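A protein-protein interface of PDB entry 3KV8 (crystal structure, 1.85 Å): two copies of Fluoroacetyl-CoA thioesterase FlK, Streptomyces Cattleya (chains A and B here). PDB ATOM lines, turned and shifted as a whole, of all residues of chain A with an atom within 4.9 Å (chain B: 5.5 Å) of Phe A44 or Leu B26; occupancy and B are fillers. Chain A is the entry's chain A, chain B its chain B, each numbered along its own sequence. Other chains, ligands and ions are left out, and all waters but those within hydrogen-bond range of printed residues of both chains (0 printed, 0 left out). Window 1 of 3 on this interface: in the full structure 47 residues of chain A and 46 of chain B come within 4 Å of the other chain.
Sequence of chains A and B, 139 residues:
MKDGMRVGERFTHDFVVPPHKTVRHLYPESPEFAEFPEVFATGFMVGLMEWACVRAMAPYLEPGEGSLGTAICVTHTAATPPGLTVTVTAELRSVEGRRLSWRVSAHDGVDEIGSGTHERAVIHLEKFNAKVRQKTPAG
The backbone carbonyl oxygen (O) of Leu B26 is in hydrogen-bond range of the side-chain amino group (NZ) of Lys A21 (3.1 Å).
NZ of Lys A21 is in salt-bridge range of OE2 of Glu B29 (2.9 Å).
The backbone carbonyl oxygen (O) of Phe A44 sits at hydrogen-bond distance from the side-chain hydroxyl (OH) of Tyr B27.
O of Lys A21 is in hydrogen-bond range of N of Ala A41, 3.1 Å away.
Among the printed residues, pairs that only touch across the chains: His A20 with Glu B29 (3.2 Å), Phe A44 with Leu B26 (3.3 Å), Gly A43 with Gly B43 (3.3 Å), Lys A21 with Tyr B27 (3.4 Å), Leu A26 with Phe B44 (3.4 Å), Gly A47 with Phe B33 (3.5 Å), Phe A40 with Tyr B27 (3.5 Å), Gly A47 with Leu B26 (3.5 Å), Leu A26 with Leu B26 (3.6 Å), Leu A48 with Tyr B27 (3.6 Å), Gly A47 with Tyr B27 (3.7 Å) and Lys A21 with Pro B28 (3.8 Å).
Phe A44 touches just these residues of chain B: Leu B26 and Tyr B27.
Leu B26 touches just these residues of chain A: Lys A21 (3.1 Å), Leu A26 (3.6 Å), Phe A44 (3.3 Å) and Gly A47 (3.5 Å).
Of the printed residues of chain B, Leu A48 touches Tyr B27 (3.6 Å).
Of the printed residues of chain B, Leu A26 touches Leu B26 and Phe B44.
His A25 touches none of the printed residues of chain B.
Arg B24 touches none of the printed residues of chain A.
The nearest residue of chain B that does not touch Phe A44 is Phe B44 (5.1 Å).
The nearest residue of chain A that does not touch Leu B26 is Gly A43 (4.1 Å).
The nearest printed residue of chain B that does not touch His A20 is Pro B28 (6.1 Å).
Printed residues of chain A that touch a printed residue of chain B: His A20, Lys A21, Leu A26, Phe A40, Gly A43, Phe A44, Gly A47 and Leu A48.
Of the 13 printed residues of chain B, 7 touch a printed residue of chain A.
Hydrophobic or aromatic side chains of chain B within 4 Å of the printed part of chain A: Leu B26, Tyr B27, Pro B28, Phe B33 and Phe B44.
Among the printed residues, 15 pairs touch across the chains.
Among the printed residues, Asp or Glu carboxylates within 4 Å of a Lys or Arg side-chain nitrogen of the other chain: Lys A21 with Glu B29 (2.9 Å).
Leu B26 touches its own counterpart, Leu A26.
Leu A26 touches Phe B44, and with the chains exchanged Phe A44 touches Leu B26.
Gly B43 touches its own counterpart, Gly A43.
7 positions are printed for both chains.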
ATOM      1  N   HIS A  20     -16.581  26.085 -16.360  1.00  0.00           N
ATOM      2  CA  HIS A  20     -17.554  27.158 -16.059  1.00  0.00           C
ATOM      3  C   HIS A  20     -18.952  26.613 -15.689  1.00  0.00           C
ATOM      4  O   HIS A  20     -19.930  27.369 -15.688  1.00  0.00           O
ATOM      5  CB  HIS A  20     -17.614  28.188 -17.199  1.00  0.00           C
ATOM      6  CG  HIS A  20     -17.872  27.561 -18.538  1.00  0.00           C
ATOM      7  ND1 HIS A  20     -19.138  27.237 -18.978  1.00  0.00           N
ATOM      8  CD2 HIS A  20     -17.013  27.109 -19.487  1.00  0.00           C
ATOM      9  CE1 HIS A  20     -19.057  26.657 -20.158  1.00  0.00           C
ATOM     10  NE2 HIS A  20     -17.778  26.593 -20.500  1.00  0.00           N
ATOM     11  N   LYS A  21     -19.013  25.316 -15.298  1.00  0.00           N
ATOM     12  CA  LYS A  21     -20.260  24.720 -14.719  1.00  0.00           C
ATOM     13  C   LYS A  21     -20.067  24.314 -13.310  1.00  0.00           C
ATOM     14  O   LYS A  21     -20.766  23.438 -12.754  1.00  0.00           O
ATOM     15  CB  LYS A  21     -20.715  23.525 -15.542  1.00  0.00           C
ATOM     16  CG  LYS A  21     -21.040  23.855 -16.954  1.00  0.00           C
ATOM     17  CD  LYS A  21     -22.239  24.791 -17.106  1.00  0.00           C
ATOM     18  CE  LYS A  21     -22.598  24.761 -18.587  1.00  0.00           C
ATOM     19  NZ  LYS A  21     -23.251  25.987 -18.967  1.00  0.00           N
ATOM     20  N   THR A  22     -19.153  24.999 -12.664  1.00  0.00           N
ATOM     21  CA  THR A  22     -18.945  24.690 -11.267  1.00  0.00           C
ATOM     22  C   THR A  22     -19.798  25.627 -10.450  1.00  0.00           C
ATOM     23  O   THR A  22     -20.454  26.603 -10.927  1.00  0.00           O
ATOM     24  CB  THR A  22     -17.455  24.776 -10.811  1.00  0.00           C
ATOM     25  OG1 THR A  22     -17.007  26.114 -10.998  1.00  0.00           O
ATOM     26  CG2 THR A  22     -16.531  23.800 -11.572  1.00  0.00           C
ATOM     27  N   HIS A  25     -19.761  29.485 -10.741  1.00  0.00           N
ATOM     28  CA  HIS A  25     -20.298  30.038 -11.982  1.00  0.00           C
ATOM     29  C   HIS A  25     -21.818  30.079 -11.997  1.00  0.00           C
ATOM     30  O   HIS A  25     -22.380  30.853 -12.781  1.00  0.00           O
ATOM     31  CB  HIS A  25     -19.787  29.210 -13.145  1.00  0.00           C
ATOM     32  CG  HIS A  25     -18.293  29.335 -13.325  1.00  0.00           C
ATOM     33  ND1 HIS A  25     -17.724  30.263 -14.178  1.00  0.00           N
ATOM     34  CD2 HIS A  25     -17.265  28.648 -12.775  1.00  0.00           C
ATOM     35  CE1 HIS A  25     -16.401  30.157 -14.121  1.00  0.00           C
ATOM     36  NE2 HIS A  25     -16.099  29.200 -13.260  1.00  0.00           N
ATOM     37  N   LEU A  26     -22.498  29.244 -11.167  1.00  0.00           N
ATOM     38  CA  LEU A  26     -23.964  29.364 -11.143  1.00  0.00           C
ATOM     39  C   LEU A  26     -24.404  30.716 -10.566  1.00  0.00           C
ATOM     40  O   LEU A  26     -25.325  31.346 -11.077  1.00  0.00           O
ATOM     41  CB  LEU A  26     -24.576  28.203 -10.301  1.00  0.00           C
ATOM     42  CG  LEU A  26     -26.096  28.008 -10.480  1.00  0.00           C
ATOM     43  CD1 LEU A  26     -26.444  27.407 -11.874  1.00  0.00           C
ATOM     44  CD2 LEU A  26     -26.529  27.047  -9.429  1.00  0.00           C
ATOM     45  N   PHE A  40     -19.161  20.284 -10.321  1.00  0.00           N
ATOM     46  CA  PHE A  40     -20.374  20.546 -11.139  1.00  0.00           C
ATOM     47  C   PHE A  40     -21.544  20.900 -10.187  1.00  0.00           C
ATOM     48  O   PHE A  40     -21.878  20.104  -9.328  1.00  0.00           O
ATOM     49  CB  PHE A  40     -20.681  19.206 -11.809  1.00  0.00           C
ATOM     50  CG  PHE A  40     -21.771  19.229 -12.896  1.00  0.00           C
ATOM     51  CD1 PHE A  40     -21.847  20.273 -13.859  1.00  0.00           C
ATOM     52  CD2 PHE A  40     -22.659  18.174 -12.977  1.00  0.00           C
ATOM     53  CE1 PHE A  40     -22.762  20.220 -14.905  1.00  0.00           C
ATOM     54  CE2 PHE A  40     -23.629  18.110 -14.021  1.00  0.00           C
ATOM     55  CZ  PHE A  40     -23.685  19.153 -14.960  1.00  0.00           C
ATOM     56  N   ALA A  41     -22.191  22.046 -10.372  1.00  0.00           N
ATOM     57  CA  ALA A  41     -23.252  22.463  -9.406  1.00  0.00           C
ATOM     58  C   ALA A  41     -24.541  21.626  -9.539  1.00  0.00           C
ATOM     59  O   ALA A  41     -24.976  21.290 -10.625  1.00  0.00           O
ATOM     60  CB  ALA A  41     -23.632  23.913  -9.656  1.00  0.00           C
ATOM     61  N   THR A  42     -25.239  21.453  -8.421  1.00  0.00           N
ATOM     62  CA  THR A  42     -26.509  20.733  -8.504  1.00  0.00           C
ATOM     63  C   THR A  42     -27.408  21.483  -9.512  1.00  0.00           C
ATOM     64  O   THR A  42     -28.088  20.880 -10.364  1.00  0.00           O
ATOM     65  CB  THR A  42     -27.193  20.624  -7.088  1.00  0.00           C
ATOM     66  OG1 THR A  42     -26.279  19.992  -6.152  1.00  0.00           O
ATOM     67  CG2 THR A  42     -28.544  19.922  -7.218  1.00  0.00           C
ATOM     68  N   GLY A  43     -27.385  22.807  -9.494  1.00  0.00           N
ATOM     69  CA  GLY A  43     -28.360  23.456 -10.407  1.00  0.00           C
ATOM     70  C   GLY A  43     -28.015  23.255 -11.892  1.00  0.00           C
ATOM     71  O   GLY A  43     -28.905  23.259 -12.749  1.00  0.00           O
ATOM     72  N   PHE A  44     -26.720  23.108 -12.222  1.00  0.00           N
ATOM     73  CA  PHE A  44     -26.320  22.729 -13.566  1.00  0.00           C
ATOM     74  C   PHE A  44     -26.661  21.288 -13.906  1.00  0.00           C
ATOM     75  O   PHE A  44     -26.995  20.985 -15.049  1.00  0.00           O
ATOM     76  CB  PHE A  44     -24.810  22.992 -13.772  1.00  0.00           C
ATOM     77  CG  PHE A  44     -24.450  24.479 -13.934  1.00  0.00           C
ATOM     78  CD1 PHE A  44     -25.078  25.239 -14.892  1.00  0.00           C
ATOM     79  CD2 PHE A  44     -23.463  25.069 -13.108  1.00  0.00           C
ATOM     80  CE1 PHE A  44     -24.721  26.613 -15.130  1.00  0.00           C
ATOM     81  CE2 PHE A  44     -23.094  26.423 -13.277  1.00  0.00           C
ATOM     82  CZ  PHE A  44     -23.743  27.205 -14.273  1.00  0.00           C
ATOM     83  N   MET A  45     -26.578  20.393 -12.915  1.00  0.00           N
ATOM     84  CA  MET A  45     -26.946  18.971 -13.119  1.00  0.00           C
ATOM     85  C   MET A  45     -28.449  18.939 -13.451  1.00  0.00           C
ATOM     86  O   MET A  45     -28.917  18.170 -14.359  1.00  0.00           O
ATOM     87  CB  MET A  45     -26.670  18.084 -11.894  1.00  0.00           C
ATOM     88  CG  MET A  45     -26.978  16.548 -12.273  1.00  0.00           C
ATOM     89  SD  MET A  45     -26.789  15.504 -10.797  1.00  0.00           S
ATOM     90  CE  MET A  45     -28.082  16.060  -9.671  1.00  0.00           C
ATOM     91  N   VAL A  46     -29.210  19.737 -12.705  1.00  0.00           N
ATOM     92  CA  VAL A  46     -30.673  19.864 -12.980  1.00  0.00           C
ATOM     93  C   VAL A  46     -30.900  20.334 -14.421  1.00  0.00           C
ATOM     94  O   VAL A  46     -31.688  19.690 -15.171  1.00  0.00           O
ATOM     95  CB  VAL A  46     -31.371  20.734 -11.929  1.00  0.00           C
ATOM     96  CG1 VAL A  46     -32.818  21.141 -12.312  1.00  0.00           C
ATOM     97  CG2 VAL A  46     -31.404  20.029 -10.608  1.00  0.00           C
ATOM     98  N   GLY A  47     -30.190  21.400 -14.788  1.00  0.00           N
ATOM     99  CA  GLY A  47     -30.306  21.999 -16.131  1.00  0.00           C
ATOM    100  C   GLY A  47     -29.990  20.901 -17.165  1.00  0.00           C
ATOM    101  O   GLY A  47     -30.653  20.816 -18.201  1.00  0.00           O
ATOM    102  N   LEU A  48     -28.950  20.096 -16.917  1.00  0.00           N
ATOM    103  CA  LEU A  48     -28.556  19.001 -17.857  1.00  0.00           C
ATOM    104  C   LEU A  48     -29.559  17.866 -17.966  1.00  0.00           C
ATOM    105  O   LEU A  48     -29.857  17.353 -19.049  1.00  0.00           O
ATOM    106  CB  LEU A  48     -27.175  18.420 -17.455  1.00  0.00           C
ATOM    107  CG  LEU A  48     -26.599  17.459 -18.474  1.00  0.00           C
ATOM    108  CD1 LEU A  48     -26.108  18.257 -19.725  1.00  0.00           C
ATOM    109  CD2 LEU A  48     -25.374  16.811 -17.821  1.00  0.00           C
ATOM    110  N   HIS B  20     -29.313  37.797 -16.853  1.00  0.00           N
ATOM    111  CA  HIS B  20     -28.431  36.631 -17.064  1.00  0.00           C
ATOM    112  C   HIS B  20     -28.809  35.361 -16.200  1.00  0.00           C
ATOM    113  O   HIS B  20     -28.022  34.411 -16.150  1.00  0.00           O
ATOM    114  CB  HIS B  20     -26.929  37.010 -16.942  1.00  0.00           C
ATOM    115  CG  HIS B  20     -26.572  37.608 -15.603  1.00  0.00           C
ATOM    116  ND1 HIS B  20     -26.715  38.954 -15.331  1.00  0.00           N
ATOM    117  CD2 HIS B  20     -26.182  37.030 -14.436  1.00  0.00           C
ATOM    118  CE1 HIS B  20     -26.362  39.189 -14.073  1.00  0.00           C
ATOM    119  NE2 HIS B  20     -26.032  38.044 -13.511  1.00  0.00           N
ATOM    120  N   THR B  22     -31.850  33.699 -16.945  1.00  0.00           N
ATOM    121  CA  THR B  22     -32.942  33.031 -17.652  1.00  0.00           C
ATOM    122  C   THR B  22     -32.391  31.720 -18.209  1.00  0.00           C
ATOM    123  O   THR B  22     -31.197  31.374 -18.112  1.00  0.00           O
ATOM    124  CB  THR B  22     -33.501  33.922 -18.786  1.00  0.00           C
ATOM    125  OG1 THR B  22     -32.408  34.232 -19.682  1.00  0.00           O
ATOM    126  CG2 THR B  22     -34.171  35.241 -18.231  1.00  0.00           C
ATOM    127  N   VAL B  23     -33.319  30.935 -18.730  1.00  0.00           N
ATOM    128  CA  VAL B  23     -33.020  29.616 -19.280  1.00  0.00           C
ATOM    129  C   VAL B  23     -31.798  29.596 -20.198  1.00  0.00           C
ATOM    130  O   VAL B  23     -30.895  28.768 -20.056  1.00  0.00           O
ATOM    131  CB  VAL B  23     -34.280  29.081 -19.999  1.00  0.00           C
ATOM    132  CG1 VAL B  23     -34.014  27.649 -20.693  1.00  0.00           C
ATOM    133  CG2 VAL B  23     -35.392  28.893 -18.955  1.00  0.00           C
ATOM    134  N   ARG B  24     -31.779  30.481 -21.202  1.00  0.00           N
ATOM    135  CA  ARG B  24     -30.673  30.467 -22.172  1.00  0.00           C
ATOM    136  C   ARG B  24     -29.267  30.629 -21.548  1.00  0.00           C
ATOM    137  O   ARG B  24     -28.244  30.118 -22.104  1.00  0.00           O
ATOM    138  CB  ARG B  24     -30.971  31.500 -23.305  1.00  0.00           C
ATOM    139  CG  ARG B  24     -30.819  32.967 -22.844  1.00  0.00           C
ATOM    140  CD  ARG B  24     -31.293  33.906 -23.969  1.00  0.00           C
ATOM    141  NE  ARG B  24     -30.352  35.013 -24.121  1.00  0.00           N
ATOM    142  CZ  ARG B  24     -30.494  36.229 -23.593  1.00  0.00           C
ATOM    143  NH1 ARG B  24     -31.555  36.543 -22.851  1.00  0.00           N
ATOM    144  NH2 ARG B  24     -29.573  37.155 -23.798  1.00  0.00           N
ATOM    145  N   HIS B  25     -29.207  31.298 -20.377  1.00  0.00           N
ATOM    146  CA  HIS B  25     -27.918  31.574 -19.715  1.00  0.00           C
ATOM    147  C   HIS B  25     -27.481  30.402 -18.862  1.00  0.00           C
ATOM    148  O   HIS B  25     -26.300  30.275 -18.522  1.00  0.00           O
ATOM    149  CB  HIS B  25     -28.092  32.760 -18.794  1.00  0.00           C
ATOM    150  CG  HIS B  25     -28.202  34.025 -19.540  1.00  0.00           C
ATOM    151  ND1 HIS B  25     -27.083  34.743 -19.927  1.00  0.00           N
ATOM    152  CD2 HIS B  25     -29.275  34.693 -20.004  1.00  0.00           C
ATOM    153  CE1 HIS B  25     -27.470  35.795 -20.629  1.00  0.00           C
ATOM    154  NE2 HIS B  25     -28.793  35.803 -20.660  1.00  0.00           N
ATOM    155  N   LEU B  26     -28.428  29.522 -18.558  1.00  0.00           N
ATOM    156  CA  LEU B  26     -28.009  28.292 -17.771  1.00  0.00           C
ATOM    157  C   LEU B  26     -27.101  27.366 -18.604  1.00  0.00           C
ATOM    158  O   LEU B  26     -26.093  26.836 -18.084  1.00  0.00           O
ATOM    159  CB  LEU B  26     -29.245  27.604 -17.124  1.00  0.00           C
ATOM    160  CG  LEU B  26     -28.888  26.455 -16.156  1.00  0.00           C
ATOM    161  CD1 LEU B  26     -28.417  26.989 -14.825  1.00  0.00           C
ATOM    162  CD2 LEU B  26     -30.098  25.529 -15.972  1.00  0.00           C
ATOM    163  N   TYR B  27     -27.487  27.157 -19.867  1.00  0.00           N
ATOM    164  CA  TYR B  27     -26.665  26.435 -20.806  1.00  0.00           C
ATOM    165  C   TYR B  27     -26.556  27.236 -22.105  1.00  0.00           C
ATOM    166  O   TYR B  27     -27.394  27.017 -23.016  1.00  0.00           O
ATOM    167  CB  TYR B  27     -27.197  25.018 -21.086  1.00  0.00           C
ATOM    168  CG  TYR B  27     -26.726  24.041 -20.015  1.00  0.00           C
ATOM    169  CD1 TYR B  27     -25.549  23.349 -20.172  1.00  0.00           C
ATOM    170  CD2 TYR B  27     -27.465  23.865 -18.841  1.00  0.00           C
ATOM    171  CE1 TYR B  27     -25.084  22.490 -19.175  1.00  0.00           C
ATOM    172  CE2 TYR B  27     -27.042  22.997 -17.830  1.00  0.00           C
ATOM    173  CZ  TYR B  27     -25.839  22.312 -18.007  1.00  0.00           C
ATOM    174  OH  TYR B  27     -25.342  21.462 -17.013  1.00  0.00           O
ATOM    175  N   PRO B  28     -25.561  28.142 -22.204  1.00  0.00           N
ATOM    176  CA  PRO B  28     -25.413  28.887 -23.492  1.00  0.00           C
ATOM    177  C   PRO B  28     -25.064  27.928 -24.631  1.00  0.00           C
ATOM    178  O   PRO B  28     -25.305  28.245 -25.806  1.00  0.00           O
ATOM    179  CB  PRO B  28     -24.237  29.838 -23.217  1.00  0.00           C
ATOM    180  CG  PRO B  28     -24.282  30.108 -21.671  1.00  0.00           C
ATOM    181  CD  PRO B  28     -24.693  28.700 -21.133  1.00  0.00           C
ATOM    182  N   GLU B  29     -24.520  26.743 -24.279  1.00  0.00           N
ATOM    183  CA  GLU B  29     -24.225  25.725 -25.274  1.00  0.00           C
ATOM    184  C   GLU B  29     -25.411  24.905 -25.825  1.00  0.00           C
ATOM    185  O   GLU B  29     -25.249  24.070 -26.725  1.00  0.00           O
ATOM    186  CB  GLU B  29     -23.038  24.824 -24.849  1.00  0.00           C
ATOM    187  CG  GLU B  29     -22.884  24.166 -23.506  1.00  0.00           C
ATOM    188  CD  GLU B  29     -22.635  25.125 -22.290  1.00  0.00           C
ATOM    189  OE1 GLU B  29     -21.485  25.283 -21.745  1.00  0.00           O
ATOM    190  OE2 GLU B  29     -23.631  25.715 -21.852  1.00  0.00           O
ATOM    191  N   PHE B  33     -32.188  25.535 -25.452  1.00  0.00           N
ATOM    192  CA  PHE B  33     -32.487  26.509 -24.371  1.00  0.00           C
ATOM    193  C   PHE B  33     -32.476  27.913 -24.921  1.00  0.00           C
ATOM    194  O   PHE B  33     -33.086  28.806 -24.329  1.00  0.00           O
ATOM    195  CB  PHE B  33     -31.480  26.445 -23.205  1.00  0.00           C
ATOM    196  CG  PHE B  33     -31.691  25.294 -22.257  1.00  0.00           C
ATOM    197  CD1 PHE B  33     -30.988  25.252 -21.047  1.00  0.00           C
ATOM    198  CD2 PHE B  33     -32.547  24.233 -22.581  1.00  0.00           C
ATOM    199  CE1 PHE B  33     -31.162  24.152 -20.128  1.00  0.00           C
ATOM    200  CE2 PHE B  33     -32.725  23.140 -21.700  1.00  0.00           C
ATOM    201  CZ  PHE B  33     -32.000  23.096 -20.489  1.00  0.00           C
ATOM    202  N   ALA B  41     -34.696  30.207 -14.795  1.00  0.00           N
ATOM    203  CA  ALA B  41     -34.529  28.751 -14.987  1.00  0.00           C
ATOM    204  C   ALA B  41     -34.663  27.994 -13.700  1.00  0.00           C
ATOM    205  O   ALA B  41     -34.201  28.449 -12.623  1.00  0.00           O
ATOM    206  CB  ALA B  41     -33.118  28.432 -15.623  1.00  0.00           C
ATOM    207  N   GLY B  43     -32.948  25.383 -12.836  1.00  0.00           N
ATOM    208  CA  GLY B  43     -31.587  25.155 -12.261  1.00  0.00           C
ATOM    209  C   GLY B  43     -31.096  26.367 -11.414  1.00  0.00           C
ATOM    210  O   GLY B  43     -30.402  26.169 -10.393  1.00  0.00           O
ATOM    211  N   PHE B  44     -31.465  27.598 -11.827  1.00  0.00           N
ATOM    212  CA  PHE B  44     -31.113  28.782 -11.071  1.00  0.00           C
ATOM    213  C   PHE B  44     -31.936  28.897  -9.801  1.00  0.00           C
ATOM    214  O   PHE B  44     -31.422  29.296  -8.783  1.00  0.00           O
ATOM    215  CB  PHE B  44     -31.144  30.087 -11.883  1.00  0.00           C
ATOM    216  CG  PHE B  44     -30.023  30.228 -12.904  1.00  0.00           C
ATOM    217  CD1 PHE B  44     -28.662  30.275 -12.516  1.00  0.00           C
ATOM    218  CD2 PHE B  44     -30.332  30.363 -14.263  1.00  0.00           C
ATOM    219  CE1 PHE B  44     -27.613  30.447 -13.495  1.00  0.00           C
ATOM    220  CE2 PHE B  44     -29.292  30.559 -15.226  1.00  0.00           C
ATOM    221  CZ  PHE B  44     -27.942  30.601 -14.843  1.00  0.00           C
